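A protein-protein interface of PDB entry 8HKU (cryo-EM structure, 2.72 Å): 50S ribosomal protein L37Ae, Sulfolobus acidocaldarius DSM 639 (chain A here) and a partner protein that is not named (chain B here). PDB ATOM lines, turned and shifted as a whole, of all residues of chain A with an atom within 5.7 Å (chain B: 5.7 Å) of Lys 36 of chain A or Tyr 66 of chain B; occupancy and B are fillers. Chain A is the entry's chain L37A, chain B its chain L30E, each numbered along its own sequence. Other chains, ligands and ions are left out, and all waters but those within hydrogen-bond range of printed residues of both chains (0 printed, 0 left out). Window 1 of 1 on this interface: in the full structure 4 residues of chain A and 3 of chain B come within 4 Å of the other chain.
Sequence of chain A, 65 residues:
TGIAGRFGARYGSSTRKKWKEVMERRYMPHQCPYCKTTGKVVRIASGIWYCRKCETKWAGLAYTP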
ATOM      1  N   GLN A  31     -15.309   8.192  -2.315  1.00  0.00           N
ATOM      2  CA  GLN A  31     -13.989   7.827  -2.804  1.00  0.00           C
ATOM      3  C   GLN A  31     -13.773   8.429  -4.182  1.00  0.00           C
ATOM      4  O   GLN A  31     -14.660   8.361  -5.035  1.00  0.00           O
ATOM      5  CB  GLN A  31     -13.831   6.311  -2.863  1.00  0.00           C
ATOM      6  CG  GLN A  31     -12.593   5.856  -3.595  1.00  0.00           C
ATOM      7  CD  GLN A  31     -12.353   4.373  -3.466  1.00  0.00           C
ATOM      8  OE1 GLN A  31     -11.219   3.925  -3.344  1.00  0.00           O
ATOM      9  NE2 GLN A  31     -13.425   3.600  -3.489  1.00  0.00           N
ATOM     10  N   CYS A  32     -12.613   9.026  -4.391  1.00  0.00           N
ATOM     11  CA  CYS A  32     -12.310   9.635  -5.678  1.00  0.00           C
ATOM     12  C   CYS A  32     -12.153   8.554  -6.738  1.00  0.00           C
ATOM     13  O   CYS A  32     -11.497   7.541  -6.486  1.00  0.00           O
ATOM     14  CB  CYS A  32     -11.040  10.466  -5.590  1.00  0.00           C
ATOM     15  SG  CYS A  32     -10.567  11.266  -7.118  1.00  0.00           S
ATOM     16  N   PRO A  33     -12.751   8.715  -7.921  1.00  0.00           N
ATOM     17  CA  PRO A  33     -12.556   7.713  -8.973  1.00  0.00           C
ATOM     18  C   PRO A  33     -11.159   7.717  -9.549  1.00  0.00           C
ATOM     19  O   PRO A  33     -10.723   6.691 -10.078  1.00  0.00           O
ATOM     20  CB  PRO A  33     -13.583   8.116 -10.038  1.00  0.00           C
ATOM     21  CG  PRO A  33     -14.459   9.116  -9.392  1.00  0.00           C
ATOM     22  CD  PRO A  33     -13.638   9.793  -8.369  1.00  0.00           C
ATOM     23  N   TYR A  34     -10.446   8.836  -9.463  1.00  0.00           N
ATOM     24  CA  TYR A  34      -9.177   9.010 -10.153  1.00  0.00           C
ATOM     25  C   TYR A  34      -7.983   8.672  -9.273  1.00  0.00           C
ATOM     26  O   TYR A  34      -7.212   7.771  -9.610  1.00  0.00           O
ATOM     27  CB  TYR A  34      -9.097  10.437 -10.691  1.00  0.00           C
ATOM     28  CG  TYR A  34     -10.261  10.731 -11.588  1.00  0.00           C
ATOM     29  CD1 TYR A  34     -10.330  10.185 -12.857  1.00  0.00           C
ATOM     30  CD2 TYR A  34     -11.313  11.516 -11.156  1.00  0.00           C
ATOM     31  CE1 TYR A  34     -11.399  10.428 -13.675  1.00  0.00           C
ATOM     32  CE2 TYR A  34     -12.390  11.762 -11.969  1.00  0.00           C
ATOM     33  CZ  TYR A  34     -12.426  11.216 -13.228  1.00  0.00           C
ATOM     34  OH  TYR A  34     -13.495  11.457 -14.051  1.00  0.00           O
ATOM     35  N   CYS A  35      -7.804   9.365  -8.150  1.00  0.00           N
ATOM     36  CA  CYS A  35      -6.676   8.979  -7.315  1.00  0.00           C
ATOM     37  C   CYS A  35      -7.033   7.835  -6.377  1.00  0.00           C
ATOM     38  O   CYS A  35      -6.576   6.718  -6.600  1.00  0.00           O
ATOM     39  CB  CYS A  35      -6.165  10.184  -6.522  1.00  0.00           C
ATOM     40  SG  CYS A  35      -7.417  11.127  -5.614  1.00  0.00           S
ATOM     41  N   LYS A  36      -7.774   8.128  -5.303  1.00  0.00           N
ATOM     42  CA  LYS A  36      -8.646   7.305  -4.452  1.00  0.00           C
ATOM     43  C   LYS A  36      -9.186   8.202  -3.348  1.00  0.00           C
ATOM     44  O   LYS A  36      -9.007   9.422  -3.391  1.00  0.00           O
ATOM     45  CB  LYS A  36      -8.026   6.054  -3.816  1.00  0.00           C
ATOM     46  CG  LYS A  36      -7.485   4.946  -4.707  1.00  0.00           C
ATOM     47  CD  LYS A  36      -8.584   4.162  -5.432  1.00  0.00           C
ATOM     48  CE  LYS A  36      -8.867   4.703  -6.817  1.00  0.00           C
ATOM     49  NZ  LYS A  36      -9.852   3.872  -7.553  1.00  0.00           N
ATOM     50  N   THR A  37      -9.773   7.605  -2.313  1.00  0.00           N
ATOM     51  CA  THR A  37     -10.439   8.335  -1.237  1.00  0.00           C
ATOM     52  C   THR A  37      -9.475   9.252  -0.500  1.00  0.00           C
ATOM     53  O   THR A  37      -9.833   9.825   0.534  1.00  0.00           O
ATOM     54  CB  THR A  37     -11.068   7.357  -0.237  1.00  0.00           C
ATOM     55  OG1 THR A  37     -11.855   8.071   0.721  1.00  0.00           O
ATOM     56  CG2 THR A  37      -9.990   6.585   0.496  1.00  0.00           C
ATOM     57  N   THR A  38      -8.246   9.358  -1.010  1.00  0.00           N
ATOM     58  CA  THR A  38      -7.154  10.088  -0.382  1.00  0.00           C
ATOM     59  C   THR A  38      -7.574  11.477   0.071  1.00  0.00           C
ATOM     60  O   THR A  38      -7.582  11.777   1.269  1.00  0.00           O
ATOM     61  CB  THR A  38      -5.990  10.258  -1.350  1.00  0.00           C
ATOM     62  OG1 THR A  38      -5.549   8.984  -1.808  1.00  0.00           O
ATOM     63  CG2 THR A  38      -4.840  10.863  -0.590  1.00  0.00           C
ATOM     64  N   GLY A  39      -7.904  12.331  -0.891  1.00  0.00           N
ATOM     65  CA  GLY A  39      -8.451  13.647  -0.612  1.00  0.00           C
ATOM     66  C   GLY A  39      -9.954  13.603  -0.818  1.00  0.00           C
ATOM     67  O   GLY A  39     -10.447  12.906  -1.706  1.00  0.00           O
ATOM     68  N   CYS A  51     -11.983  16.444  -6.317  1.00  0.00           N
ATOM     69  CA  CYS A  51     -11.169  15.908  -5.241  1.00  0.00           C
ATOM     70  C   CYS A  51     -10.102  16.918  -4.867  1.00  0.00           C
ATOM     71  O   CYS A  51      -9.460  17.507  -5.736  1.00  0.00           O
ATOM     72  CB  CYS A  51     -10.516  14.600  -5.667  1.00  0.00           C
ATOM     73  SG  CYS A  51      -9.461  13.840  -4.441  1.00  0.00           S
ATOM     74  N   THR B  38      -2.244   4.410 -10.222  1.00  0.00           N
ATOM     75  CA  THR B  38      -2.891   5.655  -9.845  1.00  0.00           C
ATOM     76  C   THR B  38      -1.907   6.801  -9.656  1.00  0.00           C
ATOM     77  O   THR B  38      -2.314   7.887  -9.237  1.00  0.00           O
ATOM     78  CB  THR B  38      -3.713   5.456  -8.574  1.00  0.00           C
ATOM     79  OG1 THR B  38      -4.663   6.517  -8.461  1.00  0.00           O
ATOM     80  CG2 THR B  38      -2.819   5.449  -7.350  1.00  0.00           C
ATOM     81  N   SER B  64      -4.012   0.581  -6.828  1.00  0.00           N
ATOM     82  CA  SER B  64      -3.646   1.944  -6.491  1.00  0.00           C
ATOM     83  C   SER B  64      -2.528   1.951  -5.453  1.00  0.00           C
ATOM     84  O   SER B  64      -2.028   0.906  -5.031  1.00  0.00           O
ATOM     85  CB  SER B  64      -4.870   2.707  -5.989  1.00  0.00           C
ATOM     86  OG  SER B  64      -5.355   2.142  -4.788  1.00  0.00           O
ATOM     87  N   GLY B  65      -2.136   3.149  -5.019  1.00  0.00           N
ATOM     88  CA  GLY B  65      -1.105   3.265  -4.009  1.00  0.00           C
ATOM     89  C   GLY B  65      -1.545   2.817  -2.638  1.00  0.00           C
ATOM     90  O   GLY B  65      -0.705   2.648  -1.753  1.00  0.00           O
ATOM     91  N   TYR B  66      -2.844   2.599  -2.446  1.00  0.00           N
ATOM     92  CA  TYR B  66      -3.337   2.169  -1.146  1.00  0.00           C
ATOM     93  C   TYR B  66      -3.209   0.670  -0.955  1.00  0.00           C
ATOM     94  O   TYR B  66      -2.741   0.214   0.092  1.00  0.00           O
ATOM     95  CB  TYR B  66      -4.779   2.605  -0.966  1.00  0.00           C
ATOM     96  CG  TYR B  66      -4.833   4.042  -0.610  1.00  0.00           C
ATOM     97  CD1 TYR B  66      -4.617   4.444   0.691  1.00  0.00           C
ATOM     98  CD2 TYR B  66      -5.054   5.000  -1.570  1.00  0.00           C
ATOM     99  CE1 TYR B  66      -4.637   5.750   1.026  1.00  0.00           C
ATOM    100  CE2 TYR B  66      -5.078   6.304  -1.242  1.00  0.00           C
ATOM    101  CZ  TYR B  66      -4.870   6.677   0.059  1.00  0.00           C
ATOM    102  OH  TYR B  66      -4.888   7.990   0.416  1.00  0.00           O
ATOM    103  N   GLU B  67      -3.643  -0.119  -1.933  1.00  0.00           N
ATOM    104  CA  GLU B  67      -3.404  -1.545  -1.796  1.00  0.00           C
ATOM    105  C   GLU B  67      -1.990  -1.942  -2.189  1.00  0.00           C
ATOM    106  O   GLU B  67      -1.629  -3.109  -2.026  1.00  0.00           O
ATOM    107  CB  GLU B  67      -4.448  -2.352  -2.573  1.00  0.00           C
ATOM    108  CG  GLU B  67      -4.500  -2.141  -4.062  1.00  0.00           C
ATOM    109  CD  GLU B  67      -5.417  -0.997  -4.433  1.00  0.00           C
ATOM    110  OE1 GLU B  67      -5.728  -0.176  -3.549  1.00  0.00           O
ATOM    111  OE2 GLU B  67      -5.859  -0.939  -5.598  1.00  0.00           O
ATOM    112  N   LEU B  68      -1.183  -1.012  -2.687  1.00  0.00           N
ATOM    113  CA  LEU B  68       0.251  -1.253  -2.735  1.00  0.00           C
ATOM    114  C   LEU B  68       0.907  -0.955  -1.396  1.00  0.00           C
ATOM    115  O   LEU B  68       1.825  -1.668  -0.983  1.00  0.00           O
ATOM    116  CB  LEU B  68       0.902  -0.419  -3.836  1.00  0.00           C
ATOM    117  CG  LEU B  68       2.342  -0.798  -4.178  1.00  0.00           C
ATOM    118  CD1 LEU B  68       2.443  -2.273  -4.486  1.00  0.00           C
ATOM    119  CD2 LEU B  68       2.837   0.021  -5.346  1.00  0.00           C
ATOM    120  N   GLY B  69       0.450   0.093  -0.707  1.00  0.00           N
ATOM    121  CA  GLY B  69       0.924   0.352   0.640  1.00  0.00           C
ATOM    122  C   GLY B  69       0.519  -0.716   1.631  1.00  0.00           C
ATOM    123  O   GLY B  69       1.271  -1.023   2.558  1.00  0.00           O
ATOM    124  N   THR B  70      -0.670  -1.295   1.456  1.00  0.00           N
ATOM    125  CA  THR B  70      -1.129  -2.346   2.354  1.00  0.00           C
ATOM    126  C   THR B  70      -0.363  -3.643   2.148  1.00  0.00           C
ATOM    127  O   THR B  70      -0.193  -4.415   3.096  1.00  0.00           O
ATOM    128  CB  THR B  70      -2.624  -2.576   2.166  1.00  0.00           C
ATOM    129  OG1 THR B  70      -3.290  -1.312   2.095  1.00  0.00           O
ATOM    130  CG2 THR B  70      -3.190  -3.362   3.325  1.00  0.00           C
ATOM    131  N   LEU B  71       0.096  -3.911   0.923  1.00  0.00           N
ATOM    132  CA  LEU B  71       0.936  -5.083   0.695  1.00  0.00           C
ATOM    133  C   LEU B  71       2.255  -4.967   1.443  1.00  0.00           C
ATOM    134  O   LEU B  71       2.736  -5.944   2.025  1.00  0.00           O
ATOM    135  CB  LEU B  71       1.186  -5.274  -0.798  1.00  0.00           C
ATOM    136  CG  LEU B  71       0.065  -5.929  -1.601  1.00  0.00           C
ATOM    137  CD1 LEU B  71       0.474  -6.071  -3.049  1.00  0.00           C
ATOM    138  CD2 LEU B  71      -0.295  -7.273  -1.009  1.00  0.00           C
ATOM    139  N   PHE B  76       0.045   3.943   5.245  1.00  0.00           N
ATOM    140  CA  PHE B  76      -0.453   4.906   4.275  1.00  0.00           C
ATOM    141  C   PHE B  76      -0.015   4.449   2.880  1.00  0.00           C
ATOM    142  O   PHE B  76       0.590   3.390   2.727  1.00  0.00           O
ATOM    143  CB  PHE B  76       0.037   6.306   4.640  1.00  0.00           C
ATOM    144  CG  PHE B  76      -0.392   7.368   3.681  1.00  0.00           C
ATOM    145  CD1 PHE B  76      -1.720   7.470   3.297  1.00  0.00           C
ATOM    146  CD2 PHE B  76       0.527   8.238   3.137  1.00  0.00           C
ATOM    147  CE1 PHE B  76      -2.121   8.435   2.405  1.00  0.00           C
ATOM    148  CE2 PHE B  76       0.131   9.197   2.248  1.00  0.00           C
ATOM    149  CZ  PHE B  76      -1.198   9.301   1.883  1.00  0.00           C
ATOM    150  N   MET B  77      -0.327   5.241   1.856  1.00  0.00           N
ATOM    151  CA  MET B  77      -0.102   4.829   0.480  1.00  0.00           C
ATOM    152  C   MET B  77       1.370   4.907   0.115  1.00  0.00           C
ATOM    153  O   MET B  77       2.095   5.789   0.578  1.00  0.00           O
ATOM    154  CB  MET B  77      -0.881   5.689  -0.515  1.00  0.00           C
ATOM    155  CG  MET B  77      -0.457   7.129  -0.595  1.00  0.00           C
ATOM    156  SD  MET B  77      -0.902   7.836  -2.191  1.00  0.00           S
ATOM    157  CE  MET B  77      -0.903   9.580  -1.829  1.00  0.00           C
ATOM    158  N   VAL B  78       1.802   3.979  -0.728  1.00  0.00           N
ATOM    159  CA  VAL B  78       3.066   4.078  -1.438  1.00  0.00           C
ATOM    160  C   VAL B  78       2.790   3.831  -2.913  1.00  0.00           C
ATOM    161  O   VAL B  78       2.135   2.849  -3.273  1.00  0.00           O
ATOM    162  CB  VAL B  78       4.125   3.108  -0.875  1.00  0.00           C
ATOM    163  CG1 VAL B  78       3.729   1.683  -1.071  1.00  0.00           C
ATOM    164  CG2 VAL B  78       5.446   3.346  -1.552  1.00  0.00           C
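The side-chain hydroxyl (OG) of Ser 64 of chain B sits close to the backbone NH (N) of Tyr 66 of chain B (3.5 Å).
OG of Ser 64 of chain B sits at hydrogen-bond distance from OE1 of Glu 67 of chain B.
The side-chain hydroxyl (OG1) of Thr 70 of chain B sits at hydrogen-bond distance from the backbone carbonyl oxygen (O) of Tyr 66 of chain B (2.6 Å).
The side-chain sulfur of Cys 32 of chain A sits close to the backbone NH of Tyr 34 of chain A (3.4 Å).
The side-chain sulfur (SG) of Cys 32 of chain A sits at hydrogen-bond distance from the side-chain sulfur (SG) of Cys 35 of chain A, 3.5 Å away.
SG of Cys 35 of chain A lies within hydrogen-bond range of SG of Cys 51 of chain A, at 3.6 Å.
The backbone carbonyl oxygen of Tyr 34 of chain A sits at hydrogen-bond distance from the side-chain hydroxyl of Thr 38 of chain B (3.1 Å).
O of Cys 35 of chain A is in hydrogen-bond range of OG1 of Thr 38 of chain B (2.7 Å).
OG1 of Thr 38 of chain A is in hydrogen-bond range of OH of Tyr 66 of chain B (2.5 Å).
Among the printed residues, merely in contact across the chains: Lys 36 of chain A with Ser 64 of chain B (3.5 Å) and Lys 36 of chain A with Tyr 66 of chain B (3.9 Å).
Of the 12 printed residues of chain B, 3 touch a printed residue of chain A.
Along chain B the printed residues that touch a printed residue of chain A span positions 38 to 66.
Of chain B, only Ser 64 (3.5 Å) and Tyr 66 (3.9 Å) come within 4 Å of Lys 36 of chain A.
Tyr 66 of chain B touches two residues of chain A.
Printed residues of chain B within 4 Å of Cys 35 of chain A: Thr 38.
Of the printed residues of chain A, Thr 38 of chain B touches Tyr 34 (3.1 Å) and Cys 35 (2.7 Å).
Printed residues of chain B within 4 Å of Thr 38 of chain A: Tyr 66 (2.5 Å).
Of the printed residues of chain B, Tyr 34 of chain A touches Thr 38.
Leu 68 of chain B touches none of the printed residues of chain A.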
